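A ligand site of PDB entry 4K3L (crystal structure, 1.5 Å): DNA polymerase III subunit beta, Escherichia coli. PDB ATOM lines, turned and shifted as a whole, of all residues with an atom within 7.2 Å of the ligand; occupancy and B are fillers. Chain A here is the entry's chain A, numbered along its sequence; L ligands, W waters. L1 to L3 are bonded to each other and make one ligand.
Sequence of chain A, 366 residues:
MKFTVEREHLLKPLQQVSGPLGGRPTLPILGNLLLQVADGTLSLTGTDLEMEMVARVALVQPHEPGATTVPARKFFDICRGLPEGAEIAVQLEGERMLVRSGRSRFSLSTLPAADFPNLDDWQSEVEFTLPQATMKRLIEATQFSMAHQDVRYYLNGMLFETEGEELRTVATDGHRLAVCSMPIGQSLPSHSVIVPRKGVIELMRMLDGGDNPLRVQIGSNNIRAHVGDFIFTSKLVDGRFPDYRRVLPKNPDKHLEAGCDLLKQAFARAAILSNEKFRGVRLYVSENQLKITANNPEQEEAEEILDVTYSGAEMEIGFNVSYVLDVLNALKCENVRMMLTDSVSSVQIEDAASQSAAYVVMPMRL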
ATOM      1  N   ARG A 152      -3.478  33.468  -9.576  1.00  0.00           N
ATOM      2  CA  ARG A 152      -3.352  33.223 -11.000  1.00  0.00           C
ATOM      3  C   ARG A 152      -4.726  33.430 -11.638  1.00  0.00           C
ATOM      4  O   ARG A 152      -5.521  32.495 -11.700  1.00  0.00           O
ATOM      5  CB  ARG A 152      -2.815  31.809 -11.238  1.00  0.00           C
ATOM      6  CG  ARG A 152      -1.430  31.605 -10.631  1.00  0.00           C
ATOM      7  CD  ARG A 152      -1.040  30.139 -10.501  1.00  0.00           C
ATOM      8  NE  ARG A 152      -1.909  29.433  -9.577  1.00  0.00           N
ATOM      9  CZ  ARG A 152      -1.783  28.158  -9.251  1.00  0.00           C
ATOM     10  NH1 ARG A 152      -0.803  27.417  -9.771  1.00  0.00           N
ATOM     11  NH2 ARG A 152      -2.654  27.617  -8.401  1.00  0.00           N
ATOM     12  N   TYR A 154      -6.205  33.791 -14.443  1.00  0.00           N
ATOM     13  CA  TYR A 154      -6.664  32.963 -15.558  1.00  0.00           C
ATOM     14  C   TYR A 154      -7.229  31.605 -15.100  1.00  0.00           C
ATOM     15  O   TYR A 154      -8.075  31.023 -15.807  1.00  0.00           O
ATOM     16  CB  TYR A 154      -5.554  32.756 -16.580  1.00  0.00           C
ATOM     17  CG  TYR A 154      -4.268  32.251 -15.988  1.00  0.00           C
ATOM     18  CD1 TYR A 154      -4.052  30.882 -15.832  1.00  0.00           C
ATOM     19  CD2 TYR A 154      -3.268  33.121 -15.576  1.00  0.00           C
ATOM     20  CE1 TYR A 154      -2.883  30.405 -15.287  1.00  0.00           C
ATOM     21  CE2 TYR A 154      -2.096  32.646 -15.017  1.00  0.00           C
ATOM     22  CZ  TYR A 154      -1.908  31.290 -14.873  1.00  0.00           C
ATOM     23  OH  TYR A 154      -0.741  30.807 -14.319  1.00  0.00           O
ATOM     24  N   LEU A 155      -6.795  31.090 -13.954  1.00  0.00           N
ATOM     25  CA  LEU A 155      -7.352  29.833 -13.427  1.00  0.00           C
ATOM     26  C   LEU A 155      -8.771  30.009 -12.879  1.00  0.00           C
ATOM     27  O   LEU A 155      -9.460  29.027 -12.639  1.00  0.00           O
ATOM     28  CB  LEU A 155      -6.473  29.245 -12.299  1.00  0.00           C
ATOM     29  CG  LEU A 155      -5.063  28.830 -12.678  1.00  0.00           C
ATOM     30  CD1 LEU A 155      -4.410  28.127 -11.491  1.00  0.00           C
ATOM     31  CD2 LEU A 155      -5.050  27.930 -13.897  1.00  0.00           C
ATOM     32  N   ALA A 171     -10.660  23.314 -17.238  1.00  0.00           N
ATOM     33  CA  ALA A 171     -10.724  24.088 -16.008  1.00  0.00           C
ATOM     34  C   ALA A 171      -9.838  23.409 -14.975  1.00  0.00           C
ATOM     35  O   ALA A 171      -9.797  22.190 -14.905  1.00  0.00           O
ATOM     36  CB  ALA A 171     -12.158  24.188 -15.517  1.00  0.00           C
ATOM     37  N   THR A 172      -9.108  24.197 -14.193  1.00  0.00           N
ATOM     38  CA  THR A 172      -8.231  23.640 -13.165  1.00  0.00           C
ATOM     39  C   THR A 172      -7.923  24.674 -12.101  1.00  0.00           C
ATOM     40  O   THR A 172      -7.941  25.886 -12.379  1.00  0.00           O
ATOM     41  CB  THR A 172      -6.928  23.105 -13.787  1.00  0.00           C
ATOM     42  OG1 THR A 172      -6.129  22.461 -12.779  1.00  0.00           O
ATOM     43  CG2 THR A 172      -6.124  24.232 -14.457  1.00  0.00           C
ATOM     44  N   ASP A 173      -7.639  24.192 -10.901  1.00  0.00           N
ATOM     45  CA  ASP A 173      -7.242  25.054  -9.794  1.00  0.00           C
ATOM     46  C   ASP A 173      -5.846  24.667  -9.275  1.00  0.00           C
ATOM     47  O   ASP A 173      -5.434  25.086  -8.188  1.00  0.00           O
ATOM     48  CB  ASP A 173      -8.297  25.005  -8.679  1.00  0.00           C
ATOM     49  CG  ASP A 173      -8.464  23.606  -8.082  1.00  0.00           C
ATOM     50  OD1 ASP A 173      -7.669  22.699  -8.410  1.00  0.00           O
ATOM     51  OD2 ASP A 173      -9.399  23.415  -7.274  1.00  0.00           O
ATOM     52  N   GLY A 174      -5.122  23.849 -10.037  1.00  0.00           N
ATOM     53  CA  GLY A 174      -3.803  23.371  -9.632  1.00  0.00           C
ATOM     54  C   GLY A 174      -3.820  22.061  -8.868  1.00  0.00           C
ATOM     55  O   GLY A 174      -2.835  21.342  -8.873  1.00  0.00           O
ATOM     56  N   HIS A 175      -4.939  21.744  -8.220  1.00  0.00           N
ATOM     57  CA  HIS A 175      -5.072  20.492  -7.451  1.00  0.00           C
ATOM     58  C   HIS A 175      -5.840  19.425  -8.233  1.00  0.00           C
ATOM     59  O   HIS A 175      -5.564  18.236  -8.092  1.00  0.00           O
ATOM     60  CB  HIS A 175      -5.771  20.750  -6.118  1.00  0.00           C
ATOM     61  CG  HIS A 175      -5.152  21.861  -5.335  1.00  0.00           C
ATOM     62  ND1 HIS A 175      -3.914  21.745  -4.737  1.00  0.00           N
ATOM     63  CD2 HIS A 175      -5.571  23.119  -5.086  1.00  0.00           C
ATOM     64  CE1 HIS A 175      -3.603  22.878  -4.130  1.00  0.00           C
ATOM     65  NE2 HIS A 175      -4.596  23.734  -4.331  1.00  0.00           N
ATOM     66  N   ARG A 176      -6.782  19.878  -9.054  1.00  0.00           N
ATOM     67  CA  ARG A 176      -7.586  18.992  -9.884  1.00  0.00           C
ATOM     68  C   ARG A 176      -7.870  19.708 -11.199  1.00  0.00           C
ATOM     69  O   ARG A 176      -7.843  20.942 -11.255  1.00  0.00           O
ATOM     70  CB  ARG A 176      -8.897  18.598  -9.183  1.00  0.00           C
ATOM     71  CG  ARG A 176      -9.576  19.682  -8.368  1.00  0.00           C
ATOM     72  CD  ARG A 176     -10.534  20.558  -9.179  1.00  0.00           C
ATOM     73  NE  ARG A 176     -11.275  21.443  -8.279  1.00  0.00           N
ATOM     74  CZ  ARG A 176     -12.375  21.111  -7.588  1.00  0.00           C
ATOM     75  NH1 ARG A 176     -12.928  19.902  -7.686  1.00  0.00           N
ATOM     76  NH2 ARG A 176     -12.937  21.999  -6.784  1.00  0.00           N
ATOM     77  N   LEU A 177      -8.105  18.932 -12.243  1.00  0.00           N
ATOM     78  CA  LEU A 177      -8.326  19.445 -13.586  1.00  0.00           C
ATOM     79  C   LEU A 177      -9.460  18.664 -14.236  1.00  0.00           C
ATOM     80  O   LEU A 177      -9.638  17.477 -13.967  1.00  0.00           O
ATOM     81  CB  LEU A 177      -7.045  19.339 -14.419  1.00  0.00           C
ATOM     82  CG  LEU A 177      -7.115  19.716 -15.907  1.00  0.00           C
ATOM     83  CD1 LEU A 177      -5.800  20.300 -16.408  1.00  0.00           C
ATOM     84  CD2 LEU A 177      -7.509  18.530 -16.795  1.00  0.00           C
ATOM     85  N   ALA A 178     -10.212  19.362 -15.087  1.00  0.00           N
ATOM     86  CA  ALA A 178     -11.255  18.782 -15.909  1.00  0.00           C
ATOM     87  C   ALA A 178     -11.055  19.231 -17.340  1.00  0.00           C
ATOM     88  O   ALA A 178     -10.769  20.399 -17.583  1.00  0.00           O
ATOM     89  CB  ALA A 178     -12.618  19.237 -15.414  1.00  0.00           C
ATOM     90  N   ARG A 240      -1.302  32.755 -19.217  1.00  0.00           N
ATOM     91  CA  ARG A 240      -0.830  31.472 -19.735  1.00  0.00           C
ATOM     92  C   ARG A 240      -1.581  30.320 -19.079  1.00  0.00           C
ATOM     93  O   ARG A 240      -1.196  29.852 -18.011  1.00  0.00           O
ATOM     94  CB  ARG A 240       0.666  31.309 -19.430  1.00  0.00           C
ATOM     95  CG  ARG A 240       1.567  32.404 -19.990  1.00  0.00           C
ATOM     96  CD  ARG A 240       2.891  31.850 -20.524  1.00  0.00           C
ATOM     97  NE  ARG A 240       4.020  31.829 -19.584  1.00  0.00           N
ATOM     98  CZ  ARG A 240       4.475  30.762 -18.937  1.00  0.00           C
ATOM     99  NH1 ARG A 240       3.895  29.572 -19.055  1.00  0.00           N
ATOM    100  NH2 ARG A 240       5.534  30.883 -18.132  1.00  0.00           N
ATOM    101  N   PHE A 241      -2.661  29.861 -19.702  1.00  0.00           N
ATOM    102  CA  PHE A 241      -3.423  28.745 -19.144  1.00  0.00           C
ATOM    103  C   PHE A 241      -2.606  27.455 -19.307  1.00  0.00           C
ATOM    104  O   PHE A 241      -2.042  27.219 -20.367  1.00  0.00           O
ATOM    105  CB  PHE A 241      -4.798  28.619 -19.804  1.00  0.00           C
ATOM    106  CG  PHE A 241      -5.805  27.909 -18.962  1.00  0.00           C
ATOM    107  CD1 PHE A 241      -5.870  26.525 -18.973  1.00  0.00           C
ATOM    108  CD2 PHE A 241      -6.663  28.607 -18.122  1.00  0.00           C
ATOM    109  CE1 PHE A 241      -6.777  25.854 -18.180  1.00  0.00           C
ATOM    110  CE2 PHE A 241      -7.579  27.941 -17.328  1.00  0.00           C
ATOM    111  CZ  PHE A 241      -7.636  26.554 -17.363  1.00  0.00           C
ATOM    112  N   PRO A 242      -2.534  26.622 -18.258  1.00  0.00           N
ATOM    113  CA  PRO A 242      -1.734  25.398 -18.399  1.00  0.00           C
ATOM    114  C   PRO A 242      -2.287  24.443 -19.465  1.00  0.00           C
ATOM    115  O   PRO A 242      -3.464  24.477 -19.768  1.00  0.00           O
ATOM    116  CB  PRO A 242      -1.808  24.755 -17.010  1.00  0.00           C
ATOM    117  CG  PRO A 242      -3.039  25.314 -16.393  1.00  0.00           C
ATOM    118  CD  PRO A 242      -3.128  26.721 -16.918  1.00  0.00           C
ATOM    119  N   ASP A 243      -1.398  23.613 -20.009  1.00  0.00           N
ATOM    120  CA  ASP A 243      -1.729  22.652 -21.038  1.00  0.00           C
ATOM    121  C   ASP A 243      -2.140  21.328 -20.398  1.00  0.00           C
ATOM    122  O   ASP A 243      -1.317  20.664 -19.757  1.00  0.00           O
ATOM    123  CB  ASP A 243      -0.501  22.448 -21.938  1.00  0.00           C
ATOM    124  CG  ASP A 243      -0.767  21.548 -23.152  1.00  0.00           C
ATOM    125  OD1 ASP A 243      -1.809  20.868 -23.224  1.00  0.00           O
ATOM    126  OD2 ASP A 243       0.082  21.532 -24.060  1.00  0.00           O
ATOM    127  N   ARG A 246      -0.083  18.094 -20.647  1.00  0.00           N
ATOM    128  CA  ARG A 246       1.066  17.898 -19.753  1.00  0.00           C
ATOM    129  C   ARG A 246       0.627  17.484 -18.346  1.00  0.00           C
ATOM    130  O   ARG A 246       1.463  17.238 -17.482  1.00  0.00           O
ATOM    131  CB  ARG A 246       1.878  19.191 -19.664  1.00  0.00           C
ATOM    132  CG  ARG A 246       2.312  19.763 -20.995  1.00  0.00           C
ATOM    133  CD  ARG A 246       3.291  18.880 -21.746  1.00  0.00           C
ATOM    134  NE  ARG A 246       4.537  18.695 -20.998  1.00  0.00           N
ATOM    135  CZ  ARG A 246       5.523  17.879 -21.359  1.00  0.00           C
ATOM    136  NH1 ARG A 246       5.436  17.145 -22.463  1.00  0.00           N
ATOM    137  NH2 ARG A 246       6.602  17.784 -20.600  1.00  0.00           N
ATOM    138  N   VAL A 247      -0.684  17.424 -18.137  1.00  0.00           N
ATOM    139  CA  VAL A 247      -1.259  17.035 -16.853  1.00  0.00           C
ATOM    140  C   VAL A 247      -1.799  15.606 -16.907  1.00  0.00           C
ATOM    141  O   VAL A 247      -1.746  14.904 -15.907  1.00  0.00           O
ATOM    142  CB  VAL A 247      -2.362  18.036 -16.428  1.00  0.00           C
ATOM    143  CG1 VAL A 247      -3.113  17.537 -15.199  1.00  0.00           C
ATOM    144  CG2 VAL A 247      -1.758  19.404 -16.171  1.00  0.00           C
ATOM    145  N   LEU A 248      -2.295  15.154 -18.067  1.00  0.00           N
ATOM    146  CA  LEU A 248      -2.772  13.781 -18.180  1.00  0.00           C
ATOM    147  C   LEU A 248      -1.605  12.846 -17.854  1.00  0.00           C
ATOM    148  O   LEU A 248      -0.520  13.026 -18.376  1.00  0.00           O
ATOM    149  CB  LEU A 248      -3.298  13.477 -19.580  1.00  0.00           C
ATOM    150  CG  LEU A 248      -4.524  14.263 -20.072  1.00  0.00           C
ATOM    151  CD1 LEU A 248      -4.835  13.874 -21.515  1.00  0.00           C
ATOM    152  CD2 LEU A 248      -5.726  13.981 -19.179  1.00  0.00           C
ATOM    153  N   SER A 346      -0.681  11.624  -9.658  1.00  0.00           N
ATOM    154  CA  SER A 346      -2.087  11.933  -9.920  1.00  0.00           C
ATOM    155  C   SER A 346      -2.842  10.735 -10.492  1.00  0.00           C
ATOM    156  O   SER A 346      -2.246   9.824 -11.043  1.00  0.00           O
ATOM    157  CB  SER A 346      -2.173  13.104 -10.902  1.00  0.00           C
ATOM    158  OG  SER A 346      -1.499  12.782 -12.101  1.00  0.00           O
ATOM    159  N   VAL A 347      -4.162  10.791 -10.360  1.00  0.00           N
ATOM    160  CA  VAL A 347      -5.071   9.784 -10.920  1.00  0.00           C
ATOM    161  C   VAL A 347      -5.875  10.455 -12.019  1.00  0.00           C
ATOM    162  O   VAL A 347      -6.178  11.641 -11.935  1.00  0.00           O
ATOM    163  CB  VAL A 347      -6.016   9.200  -9.842  1.00  0.00           C
ATOM    164  CG1 VAL A 347      -6.952  10.261  -9.263  1.00  0.00           C
ATOM    165  CG2 VAL A 347      -6.826   8.045 -10.403  1.00  0.00           C
ATOM    166  N   VAL A 360      -8.350  14.866 -13.689  1.00  0.00           N
ATOM    167  CA  VAL A 360      -7.061  14.541 -13.078  1.00  0.00           C
ATOM    168  C   VAL A 360      -7.056  15.148 -11.679  1.00  0.00           C
ATOM    169  O   VAL A 360      -7.418  16.312 -11.469  1.00  0.00           O
ATOM    170  CB  VAL A 360      -5.864  15.076 -13.891  1.00  0.00           C
ATOM    171  CG1 VAL A 360      -4.550  14.704 -13.219  1.00  0.00           C
ATOM    172  CG2 VAL A 360      -5.911  14.559 -15.320  1.00  0.00           C
ATOM    173  N   VAL A 361      -6.683  14.324 -10.707  1.00  0.00           N
ATOM    174  CA  VAL A 361      -6.666  14.736  -9.319  1.00  0.00           C
ATOM    175  C   VAL A 361      -5.332  14.402  -8.680  1.00  0.00           C
ATOM    176  O   VAL A 361      -4.849  13.275  -8.818  1.00  0.00           O
ATOM    177  CB  VAL A 361      -7.791  14.049  -8.516  1.00  0.00           C
ATOM    178  CG1 VAL A 361      -7.808  14.536  -7.083  1.00  0.00           C
ATOM    179  CG2 VAL A 361      -9.141  14.264  -9.190  1.00  0.00           C
ATOM    180  N   MET A 362      -4.757  15.373  -7.973  1.00  0.00           N
ATOM    181  CA  MET A 362      -3.500  15.173  -7.253  1.00  0.00           C
ATOM    182  C   MET A 362      -3.683  14.207  -6.093  1.00  0.00           C
ATOM    183  O   MET A 362      -4.714  14.215  -5.454  1.00  0.00           O
ATOM    184  CB  MET A 362      -3.009  16.493  -6.665  1.00  0.00           C
ATOM    185  CG  MET A 362      -2.280  17.367  -7.655  1.00  0.00           C
ATOM    186  SD  MET A 362      -0.703  16.658  -8.111  1.00  0.00           S
ATOM    187  CE  MET A 362       0.267  16.970  -6.627  1.00  0.00           C
ATOM    188  N   PRO A 363      -2.652  13.399  -5.798  1.00  0.00           N
ATOM    189  CA  PRO A 363      -2.707  12.617  -4.564  1.00  0.00           C
ATOM    190  C   PRO A 363      -2.367  13.483  -3.351  1.00  0.00           C
ATOM    191  O   PRO A 363      -1.819  14.569  -3.509  1.00  0.00           O
ATOM    192  CB  PRO A 363      -1.617  11.581  -4.790  1.00  0.00           C
ATOM    193  CG  PRO A 363      -0.610  12.288  -5.610  1.00  0.00           C
ATOM    194  CD  PRO A 363      -1.348  13.267  -6.477  1.00  0.00           C
HETATM  195  C1  LIG L   1       0.573  19.949  -9.013  1.00  0.00           C
HETATM  196  O1  LIG L   1       1.568  19.294  -9.295  1.00  0.00           O
HETATM  197  C2  LIG L   1       0.488  20.607  -7.641  1.00  0.00           C
HETATM  198  N1  LG2 L   2      -0.506  20.035  -9.835  1.00  0.00           N
HETATM  199  C1  LG2 L   2      -0.505  19.476 -11.230  1.00  0.00           C
HETATM  200  C2  LG2 L   2       0.431  20.187 -12.204  1.00  0.00           C
HETATM  201  O1  LG2 L   2       0.786  19.635 -13.232  1.00  0.00           O
HETATM  202  C3  LG2 L   2      -1.929  19.492 -11.810  1.00  0.00           C
HETATM  203  C4  LG2 L   2      -2.944  18.629 -11.078  1.00  0.00           C
HETATM  204  C5  LG2 L   2      -4.354  18.896 -11.610  1.00  0.00           C
HETATM  205  C6  LG2 L   2      -2.605  17.158 -11.207  1.00  0.00           C
HETATM  206  N1  LG3 L   3       0.755  21.446 -11.886  1.00  0.00           N
HETATM  207  C1  LG3 L   3       1.638  22.295 -12.691  1.00  0.00           C
HETATM  208  C2  LG3 L   3       2.137  23.444 -11.810  1.00  0.00           C
HETATM  209  O1  LG3 L   3       1.706  23.613 -10.662  1.00  0.00           O
HETATM  210  C3  LG3 L   3       0.878  22.860 -13.898  1.00  0.00           C
HETATM  211  C4  LG3 L   3      -0.423  23.519 -13.533  1.00  0.00           C
HETATM  212  C5  LG3 L   3      -0.459  24.847 -13.132  1.00  0.00           C
HETATM  213  C6  LG3 L   3      -1.610  22.802 -13.554  1.00  0.00           C
HETATM  214  C7  LG3 L   3      -1.642  25.452 -12.782  1.00  0.00           C
HETATM  215  C8  LG3 L   3      -2.806  23.405 -13.208  1.00  0.00           C
HETATM  216  C9  LG3 L   3      -2.823  24.728 -12.817  1.00  0.00           C
HETATM  217  O2  LG3 L   3       2.957  24.263 -12.239  1.00  0.00           O
HETATM  218  O   HOH W   1      -0.576  24.536  -9.260  1.00  0.00           O
HETATM  219  O   HOH W   2       2.056  19.725 -15.767  1.00  0.00           O
HETATM  220  O   HOH W   3       1.098  16.960 -13.486  1.00  0.00           O
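Water W1 lies within hydrogen-bond range of O1 of LG3 L3 and NH1 of Arg 152. Water W2 bridges an oxygen (O1) of LG2 L2 and the backbone carbonyl oxygen of Arg 246.
The backbone carbonyl oxygen (O) of Gly 174 sits at hydrogen-bond distance from a nitrogen (N1) of LG2 L2 (2.8 Å). SD of Met 362 lies close to N1 of LG2 L2 (3.8 Å).
The backbone NH (N) of Gly 174 is in hydrogen-bond range of the side-chain hydroxyl (OG1) of Thr 172 (3.2 Å). OG1 of Thr 172 sits at hydrogen-bond distance from O of Arg 176, 2.8 Å away. The backbone NH (N) of Met 362 is in hydrogen-bond range of the backbone carbonyl oxygen (O) of His 175 (3.0 Å). The guanidinium group (NE) of Arg 176 lies within salt-bridge range of the side-chain carboxylate (OD2) of Asp 173, 2.9 Å away. O of Val 360 sits at hydrogen-bond distance from N of Leu 177, at 2.8 Å. The backbone NH (N) of His 175 lies within hydrogen-bond range of the side-chain carboxylate (OD1) of Asp 173 (2.9 Å).
Residues that only touch the ligand: Arg 152 (3.7 Å), Leu 155 (3.98 Å), Thr 172 (3.5 Å), His 175 (3.7 Å), Arg 176 (3.6 Å), Leu 177 (3.8 Å), Pro 242 (3.6 Å), Val 247 (3.9 Å) and Val 360 (3.7 Å). Hydrophobic or aromatic side chains that line the ligand: Leu 155, Leu 177, Pro 242, Val 247, Val 360 and Met 362.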
